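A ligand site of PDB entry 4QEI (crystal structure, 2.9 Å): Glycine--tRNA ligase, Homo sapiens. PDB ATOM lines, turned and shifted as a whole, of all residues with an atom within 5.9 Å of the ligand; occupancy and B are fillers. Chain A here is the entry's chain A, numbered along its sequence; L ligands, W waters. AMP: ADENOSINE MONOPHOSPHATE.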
ATOM      1  N   PRO A 181      15.523  19.013 -13.699  1.00  0.00           N
ATOM      2  CA  PRO A 181      16.761  18.597 -13.031  1.00  0.00           C
ATOM      3  C   PRO A 181      17.286  17.235 -13.499  1.00  0.00           C
ATOM      4  O   PRO A 181      18.394  16.833 -13.144  1.00  0.00           O
ATOM      5  CB  PRO A 181      16.363  18.567 -11.567  1.00  0.00           C
ATOM      6  CG  PRO A 181      14.920  18.176 -11.615  1.00  0.00           C
ATOM      7  CD  PRO A 181      14.339  18.779 -12.850  1.00  0.00           C
ATOM      8  N   GLU A 182      16.512  16.574 -14.355  1.00  0.00           N
ATOM      9  CA  GLU A 182      16.852  15.276 -14.947  1.00  0.00           C
ATOM     10  C   GLU A 182      16.003  15.095 -16.227  1.00  0.00           C
ATOM     11  O   GLU A 182      15.053  15.851 -16.461  1.00  0.00           O
ATOM     12  CB  GLU A 182      16.662  14.146 -13.948  1.00  0.00           C
ATOM     13  CG  GLU A 182      15.226  13.868 -13.636  1.00  0.00           C
ATOM     14  CD  GLU A 182      15.021  12.719 -12.673  1.00  0.00           C
ATOM     15  OE1 GLU A 182      13.894  12.180 -12.651  1.00  0.00           O
ATOM     16  OE2 GLU A 182      15.987  12.306 -12.006  1.00  0.00           O
ATOM     17  N   ARG A 214      20.703  22.144 -12.099  1.00  0.00           N
ATOM     18  CA  ARG A 214      20.781  21.937 -10.679  1.00  0.00           C
ATOM     19  C   ARG A 214      21.382  23.149 -10.032  1.00  0.00           C
ATOM     20  O   ARG A 214      22.523  23.447 -10.313  1.00  0.00           O
ATOM     21  CB  ARG A 214      21.661  20.720 -10.346  1.00  0.00           C
ATOM     22  CG  ARG A 214      21.323  19.433 -11.022  1.00  0.00           C
ATOM     23  CD  ARG A 214      20.565  18.517 -10.125  1.00  0.00           C
ATOM     24  NE  ARG A 214      20.204  17.345 -10.904  1.00  0.00           N
ATOM     25  CZ  ARG A 214      20.455  16.095 -10.557  1.00  0.00           C
ATOM     26  NH1 ARG A 214      21.084  15.852  -9.415  1.00  0.00           N
ATOM     27  NH2 ARG A 214      20.102  15.109 -11.354  1.00  0.00           N
ATOM     28  N   GLU A 216      23.046  24.465  -7.818  1.00  0.00           N
ATOM     29  CA  GLU A 216      24.027  24.105  -6.791  1.00  0.00           C
ATOM     30  C   GLU A 216      24.523  25.179  -5.812  1.00  0.00           C
ATOM     31  O   GLU A 216      24.805  26.314  -6.184  1.00  0.00           O
ATOM     32  CB  GLU A 216      25.250  23.471  -7.441  1.00  0.00           C
ATOM     33  CG  GLU A 216      24.965  22.174  -8.166  1.00  0.00           C
ATOM     34  CD  GLU A 216      24.424  21.076  -7.255  1.00  0.00           C
ATOM     35  OE1 GLU A 216      24.174  21.345  -6.051  1.00  0.00           O
ATOM     36  OE2 GLU A 216      24.244  19.933  -7.747  1.00  0.00           O
ATOM     37  N   LEU A 223      34.411  20.367 -13.650  1.00  0.00           N
ATOM     38  CA  LEU A 223      33.256  19.772 -14.347  1.00  0.00           C
ATOM     39  C   LEU A 223      32.431  18.779 -13.464  1.00  0.00           C
ATOM     40  O   LEU A 223      31.341  18.352 -13.847  1.00  0.00           O
ATOM     41  CB  LEU A 223      33.726  19.045 -15.608  1.00  0.00           C
ATOM     42  CG  LEU A 223      34.082  19.740 -16.923  1.00  0.00           C
ATOM     43  CD1 LEU A 223      34.545  18.690 -17.921  1.00  0.00           C
ATOM     44  CD2 LEU A 223      32.973  20.605 -17.512  1.00  0.00           C
ATOM     45  N   ILE A 224      32.985  18.344 -12.339  1.00  0.00           N
ATOM     46  CA  ILE A 224      32.334  17.318 -11.588  1.00  0.00           C
ATOM     47  C   ILE A 224      31.060  17.777 -10.881  1.00  0.00           C
ATOM     48  O   ILE A 224      30.078  17.029 -10.819  1.00  0.00           O
ATOM     49  CB  ILE A 224      33.320  16.787 -10.520  1.00  0.00           C
ATOM     50  CG1 ILE A 224      34.490  16.108 -11.205  1.00  0.00           C
ATOM     51  CG2 ILE A 224      32.647  15.805  -9.573  1.00  0.00           C
ATOM     52  CD1 ILE A 224      35.478  15.537 -10.247  1.00  0.00           C
ATOM     53  N   ARG A 225      31.059  18.983 -10.317  1.00  0.00           N
ATOM     54  CA  ARG A 225      29.833  19.462  -9.688  1.00  0.00           C
ATOM     55  C   ARG A 225      29.516  20.813 -10.345  1.00  0.00           C
ATOM     56  O   ARG A 225      30.034  21.841  -9.903  1.00  0.00           O
ATOM     57  CB  ARG A 225      29.943  19.515  -8.178  1.00  0.00           C
ATOM     58  CG  ARG A 225      28.583  19.431  -7.541  1.00  0.00           C
ATOM     59  CD  ARG A 225      28.665  19.016  -6.076  1.00  0.00           C
ATOM     60  NE  ARG A 225      27.414  19.260  -5.365  1.00  0.00           N
ATOM     61  CZ  ARG A 225      26.410  18.368  -5.330  1.00  0.00           C
ATOM     62  NH1 ARG A 225      25.278  18.641  -4.680  1.00  0.00           N
ATOM     63  NH2 ARG A 225      26.541  17.206  -5.963  1.00  0.00           N
ATOM     64  N   VAL A 226      28.679  20.789 -11.363  1.00  0.00           N
ATOM     65  CA  VAL A 226      28.317  21.934 -12.214  1.00  0.00           C
ATOM     66  C   VAL A 226      26.823  22.173 -12.115  1.00  0.00           C
ATOM     67  O   VAL A 226      26.139  21.387 -11.472  1.00  0.00           O
ATOM     68  CB  VAL A 226      28.685  21.785 -13.709  1.00  0.00           C
ATOM     69  CG1 VAL A 226      30.191  21.635 -13.883  1.00  0.00           C
ATOM     70  CG2 VAL A 226      27.986  20.617 -14.337  1.00  0.00           C
ATOM     71  N   ARG A 227      26.359  23.322 -12.585  1.00  0.00           N
ATOM     72  CA  ARG A 227      24.944  23.700 -12.463  1.00  0.00           C
ATOM     73  C   ARG A 227      24.133  23.275 -13.719  1.00  0.00           C
ATOM     74  O   ARG A 227      22.926  23.213 -13.634  1.00  0.00           O
ATOM     75  CB  ARG A 227      24.826  25.185 -12.193  1.00  0.00           C
ATOM     76  CG  ARG A 227      25.416  25.620 -10.869  1.00  0.00           C
ATOM     77  CD  ARG A 227      25.183  27.099 -10.736  1.00  0.00           C
ATOM     78  NE  ARG A 227      25.185  27.625  -9.382  1.00  0.00           N
ATOM     79  CZ  ARG A 227      25.812  28.742  -9.032  1.00  0.00           C
ATOM     80  NH1 ARG A 227      26.556  29.394  -9.916  1.00  0.00           N
ATOM     81  NH2 ARG A 227      25.766  29.174  -7.783  1.00  0.00           N
ATOM     82  N   PHE A 229      24.438  20.373 -17.076  1.00  0.00           N
ATOM     83  CA  PHE A 229      25.330  19.283 -17.518  1.00  0.00           C
ATOM     84  C   PHE A 229      24.499  18.432 -18.440  1.00  0.00           C
ATOM     85  O   PHE A 229      23.280  18.459 -18.356  1.00  0.00           O
ATOM     86  CB  PHE A 229      25.967  18.475 -16.373  1.00  0.00           C
ATOM     87  CG  PHE A 229      25.027  18.040 -15.314  1.00  0.00           C
ATOM     88  CD1 PHE A 229      24.376  16.822 -15.409  1.00  0.00           C
ATOM     89  CD2 PHE A 229      24.672  18.916 -14.314  1.00  0.00           C
ATOM     90  CE1 PHE A 229      23.507  16.436 -14.442  1.00  0.00           C
ATOM     91  CE2 PHE A 229      23.771  18.559 -13.364  1.00  0.00           C
ATOM     92  CZ  PHE A 229      23.187  17.311 -13.421  1.00  0.00           C
ATOM     93  N   MET A 231      23.145  14.998 -19.742  1.00  0.00           N
ATOM     94  CA  MET A 231      22.859  13.654 -19.255  1.00  0.00           C
ATOM     95  C   MET A 231      22.379  12.771 -20.369  1.00  0.00           C
ATOM     96  O   MET A 231      21.653  13.193 -21.258  1.00  0.00           O
ATOM     97  CB  MET A 231      21.735  13.725 -18.207  1.00  0.00           C
ATOM     98  CG  MET A 231      22.093  14.599 -17.051  1.00  0.00           C
ATOM     99  SD  MET A 231      23.443  13.727 -16.240  1.00  0.00           S
ATOM    100  CE  MET A 231      22.395  12.319 -15.847  1.00  0.00           C
ATOM    101  N   GLU A 233      20.147   9.415 -20.277  1.00  0.00           N
ATOM    102  CA  GLU A 233      19.369   8.577 -19.360  1.00  0.00           C
ATOM    103  C   GLU A 233      18.569   7.502 -20.089  1.00  0.00           C
ATOM    104  O   GLU A 233      17.891   7.746 -21.081  1.00  0.00           O
ATOM    105  CB  GLU A 233      18.429   9.436 -18.498  1.00  0.00           C
ATOM    106  CG  GLU A 233      19.152  10.279 -17.425  1.00  0.00           C
ATOM    107  CD  GLU A 233      18.170  10.974 -16.496  1.00  0.00           C
ATOM    108  OE1 GLU A 233      17.192  11.575 -16.988  1.00  0.00           O
ATOM    109  OE2 GLU A 233      18.268  10.776 -15.251  1.00  0.00           O
ATOM    110  N   GLU A 340      31.230   9.178  -9.076  1.00  0.00           N
ATOM    111  CA  GLU A 340      30.157   8.493  -9.805  1.00  0.00           C
ATOM    112  C   GLU A 340      29.964   9.146 -11.198  1.00  0.00           C
ATOM    113  O   GLU A 340      29.760  10.369 -11.360  1.00  0.00           O
ATOM    114  CB  GLU A 340      28.892   8.466  -8.928  1.00  0.00           C
ATOM    115  CG  GLU A 340      27.680   7.803  -9.522  1.00  0.00           C
ATOM    116  CD  GLU A 340      26.378   8.543  -9.163  1.00  0.00           C
ATOM    117  OE1 GLU A 340      26.344   9.148  -8.066  1.00  0.00           O
ATOM    118  OE2 GLU A 340      25.375   8.490  -9.942  1.00  0.00           O
ATOM    119  N   ILE A 341      29.966   8.285 -12.212  1.00  0.00           N
ATOM    120  CA  ILE A 341      29.852   8.736 -13.595  1.00  0.00           C
ATOM    121  C   ILE A 341      28.568   8.130 -14.181  1.00  0.00           C
ATOM    122  O   ILE A 341      27.948   8.681 -15.111  1.00  0.00           O
ATOM    123  CB  ILE A 341      31.091   8.423 -14.442  1.00  0.00           C
ATOM    124  CG1 ILE A 341      31.472   6.958 -14.427  1.00  0.00           C
ATOM    125  CG2 ILE A 341      32.224   9.267 -13.957  1.00  0.00           C
ATOM    126  CD1 ILE A 341      32.729   6.678 -15.205  1.00  0.00           C
ATOM    127  N   VAL A 342      28.167   6.996 -13.658  1.00  0.00           N
ATOM    128  CA  VAL A 342      26.922   6.426 -14.135  1.00  0.00           C
ATOM    129  C   VAL A 342      26.185   6.016 -12.876  1.00  0.00           C
ATOM    130  O   VAL A 342      26.525   5.048 -12.246  1.00  0.00           O
ATOM    131  CB  VAL A 342      27.177   5.190 -14.981  1.00  0.00           C
ATOM    132  CG1 VAL A 342      25.896   4.679 -15.504  1.00  0.00           C
ATOM    133  CG2 VAL A 342      28.103   5.530 -16.153  1.00  0.00           C
ATOM    134  N   GLY A 343      25.013   6.595 -12.737  1.00  0.00           N
ATOM    135  CA  GLY A 343      24.065   6.336 -11.682  1.00  0.00           C
ATOM    136  C   GLY A 343      23.129   5.234 -12.065  1.00  0.00           C
ATOM    137  O   GLY A 343      22.838   5.022 -13.241  1.00  0.00           O
ATOM    138  N   GLU A 459      17.104   2.361 -14.356  1.00  0.00           N
ATOM    139  CA  GLU A 459      17.495   3.689 -14.796  1.00  0.00           C
ATOM    140  C   GLU A 459      18.981   3.948 -14.705  1.00  0.00           C
ATOM    141  O   GLU A 459      19.457   4.336 -13.627  1.00  0.00           O
ATOM    142  CB  GLU A 459      16.760   4.775 -14.036  1.00  0.00           C
ATOM    143  CG  GLU A 459      17.094   6.148 -14.581  1.00  0.00           C
ATOM    144  CD  GLU A 459      17.342   7.185 -13.507  1.00  0.00           C
ATOM    145  OE1 GLU A 459      16.636   8.235 -13.584  1.00  0.00           O
ATOM    146  OE2 GLU A 459      18.219   6.962 -12.608  1.00  0.00           O
ATOM    147  N   SER A 461      21.904   6.303 -15.617  1.00  0.00           N
ATOM    148  CA  SER A 461      22.020   7.748 -15.766  1.00  0.00           C
ATOM    149  C   SER A 461      23.482   8.161 -15.949  1.00  0.00           C
ATOM    150  O   SER A 461      24.254   8.173 -15.001  1.00  0.00           O
ATOM    151  CB  SER A 461      21.429   8.397 -14.520  1.00  0.00           C
ATOM    152  OG  SER A 461      21.336   9.787 -14.607  1.00  0.00           O
ATOM    153  N   PHE A 462      23.826   8.578 -17.164  1.00  0.00           N
ATOM    154  CA  PHE A 462      25.210   8.886 -17.577  1.00  0.00           C
ATOM    155  C   PHE A 462      25.539  10.381 -17.513  1.00  0.00           C
ATOM    156  O   PHE A 462      24.949  11.200 -18.257  1.00  0.00           O
ATOM    157  CB  PHE A 462      25.435   8.428 -19.022  1.00  0.00           C
ATOM    158  CG  PHE A 462      25.273   6.948 -19.269  1.00  0.00           C
ATOM    159  CD1 PHE A 462      24.007   6.340 -19.161  1.00  0.00           C
ATOM    160  CD2 PHE A 462      26.342   6.185 -19.700  1.00  0.00           C
ATOM    161  CE1 PHE A 462      23.828   5.002 -19.445  1.00  0.00           C
ATOM    162  CE2 PHE A 462      26.183   4.827 -19.968  1.00  0.00           C
ATOM    163  CZ  PHE A 462      24.911   4.221 -19.836  1.00  0.00           C
ATOM    164  N   GLY A 463      26.517  10.751 -16.699  1.00  0.00           N
ATOM    165  CA  GLY A 463      26.991  12.135 -16.639  1.00  0.00           C
ATOM    166  C   GLY A 463      28.152  12.413 -17.602  1.00  0.00           C
ATOM    167  O   GLY A 463      29.320  12.255 -17.257  1.00  0.00           O
ATOM    168  N   LEU A 464      27.810  12.850 -18.811  1.00  0.00           N
ATOM    169  CA  LEU A 464      28.760  13.008 -19.905  1.00  0.00           C
ATOM    170  C   LEU A 464      29.915  13.895 -19.491  1.00  0.00           C
ATOM    171  O   LEU A 464      31.032  13.688 -19.944  1.00  0.00           O
ATOM    172  CB  LEU A 464      28.061  13.561 -21.149  1.00  0.00           C
ATOM    173  CG  LEU A 464      26.815  12.732 -21.611  1.00  0.00           C
ATOM    174  CD1 LEU A 464      26.127  13.310 -22.843  1.00  0.00           C
ATOM    175  CD2 LEU A 464      27.029  11.230 -21.793  1.00  0.00           C
ATOM    176  N   ARG A 466      31.328  14.264 -16.437  1.00  0.00           N
ATOM    177  CA  ARG A 466      32.197  13.505 -15.583  1.00  0.00           C
ATOM    178  C   ARG A 466      32.896  12.421 -16.396  1.00  0.00           C
ATOM    179  O   ARG A 466      34.061  12.134 -16.187  1.00  0.00           O
ATOM    180  CB  ARG A 466      31.405  12.921 -14.434  1.00  0.00           C
ATOM    181  CG  ARG A 466      30.868  13.981 -13.504  1.00  0.00           C
ATOM    182  CD  ARG A 466      30.082  13.395 -12.378  1.00  0.00           C
ATOM    183  NE  ARG A 466      29.794  14.381 -11.352  1.00  0.00           N
ATOM    184  CZ  ARG A 466      29.301  14.084 -10.172  1.00  0.00           C
ATOM    185  NH1 ARG A 466      29.040  12.818  -9.904  1.00  0.00           N
ATOM    186  NH2 ARG A 466      29.054  15.025  -9.287  1.00  0.00           N
HETATM  187  P   AMP L   1      21.585  11.904 -10.159  1.00  0.00           P
HETATM  188  O1P AMP L   1      21.528  10.563  -9.450  1.00  0.00           O
HETATM  189  O2P AMP L   1      20.511  12.120 -11.212  1.00  0.00           O
HETATM  190  O3P AMP L   1      21.768  13.083  -9.224  1.00  0.00           O
HETATM  191  O5' AMP L   1      22.953  11.808 -10.966  1.00  0.00           O
HETATM  192  C5' AMP L   1      23.062  11.096 -12.201  1.00  0.00           C
HETATM  193  C4' AMP L   1      24.411  11.307 -12.843  1.00  0.00           C
HETATM  194  O4' AMP L   1      24.490  12.669 -13.306  1.00  0.00           O
HETATM  195  C3' AMP L   1      25.606  11.127 -11.915  1.00  0.00           C
HETATM  196  O3' AMP L   1      26.096   9.795 -11.898  1.00  0.00           O
HETATM  197  C2' AMP L   1      26.644  12.140 -12.425  1.00  0.00           C
HETATM  198  O2' AMP L   1      27.447  11.575 -13.445  1.00  0.00           O
HETATM  199  C1' AMP L   1      25.771  13.213 -13.050  1.00  0.00           C
HETATM  200  N9  AMP L   1      25.609  14.408 -12.200  1.00  0.00           N
HETATM  201  C8  AMP L   1      24.726  14.552 -11.181  1.00  0.00           C
HETATM  202  N7  AMP L   1      24.807  15.796 -10.633  1.00  0.00           N
HETATM  203  C5  AMP L   1      25.756  16.453 -11.327  1.00  0.00           C
HETATM  204  C6  AMP L   1      26.354  17.800 -11.264  1.00  0.00           C
HETATM  205  N6  AMP L   1      25.913  18.671 -10.326  1.00  0.00           N
HETATM  206  N1  AMP L   1      27.331  18.104 -12.151  1.00  0.00           N
HETATM  207  C2  AMP L   1      27.742  17.205 -13.082  1.00  0.00           C
HETATM  208  N3  AMP L   1      27.248  15.963 -13.209  1.00  0.00           N
HETATM  209  C4  AMP L   1      26.279  15.542 -12.359  1.00  0.00           C
HETATM  210  O   HOH W   1      28.480  15.204 -15.530  1.00  0.00           O
HETATM  211  O   HOH W   2      18.735  10.611 -12.190  1.00  0.00           O
HETATM  212  O   HOH W   3      24.262  13.157  -7.142  1.00  0.00           O
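A nitrogen (N6) of the ligand lies within hydrogen-bond range of the side-chain carboxylate (OE2) of Glu 216, at 3.3 Å. The backbone carbonyl oxygen of Val 226 is in hydrogen-bond range of a nitrogen (N6) of the ligand (3.0 Å). N of Gly 343 lies within hydrogen-bond range of O3' of the ligand (3.5 Å). The backbone carbonyl oxygen (O) of Glu 340 is in hydrogen-bond range of an oxygen (O2') of the ligand, 3.3 Å away. The guanidinium group of Arg 214 lies within salt-bridge range of an oxygen (O3P) of the ligand (2.9 Å). An oxygen (O2') of the ligand sits at hydrogen-bond distance from the backbone carbonyl oxygen (O) of Ile 341 (3.4 Å). N of Gly 463 lies close to O2' of the ligand, 3.5 Å away. N of Val 226 sits at hydrogen-bond distance from N1 of the ligand, 3.1 Å away. The side-chain carboxylate of Glu 340 is in hydrogen-bond range of an oxygen (O3') of the ligand.
The backbone NH (N) of Gly 343 lies close to the side-chain carboxylate (OE2) of Glu 340 (3.4 Å). The guanidinium group (NH1) of Arg 225 lies within salt-bridge range of the side-chain carboxylate (OE1) of Glu 216, at 3.2 Å. The backbone carbonyl oxygen of Glu 216 sits at hydrogen-bond distance from the guanidinium group of Arg 227, at 3.4 Å. The backbone carbonyl oxygen of Glu 340 lies within hydrogen-bond range of the guanidinium group of Arg 466 (2.9 Å). O of Ile 341 lies within hydrogen-bond range of N of Gly 463, 3.0 Å away. The side-chain hydroxyl of Ser 461 lies within hydrogen-bond range of the side-chain carboxylate of Glu 233 (3.3 Å). The guanidinium group (NE) of Arg 214 is in hydrogen-bond range of the backbone carbonyl oxygen (O) of Pro 181 (2.9 Å). NE of Arg 466 is in hydrogen-bond range of O of Ile 224 (2.7 Å).
O of Ile 224 sits close to N1 of the ligand (3.2 Å). O4' of the ligand sits close to SD of Met 231 (3.3 Å). Residues that only touch the ligand: Leu 223, Arg 225, Phe 229, Val 342, Ser 461 and Arg 466. Hydrophobic or aromatic side chains within 4 Å of the ligand: Val 226, Phe 229 and Met 231. Of the 22 residues printed, 15 come within 4 Å of the ligand. Along chain A the residues within 4 Å of the ligand span positions 214 to 466.
Water W1 lies within hydrogen-bond range of N3 of the ligand and N of Arg 466.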
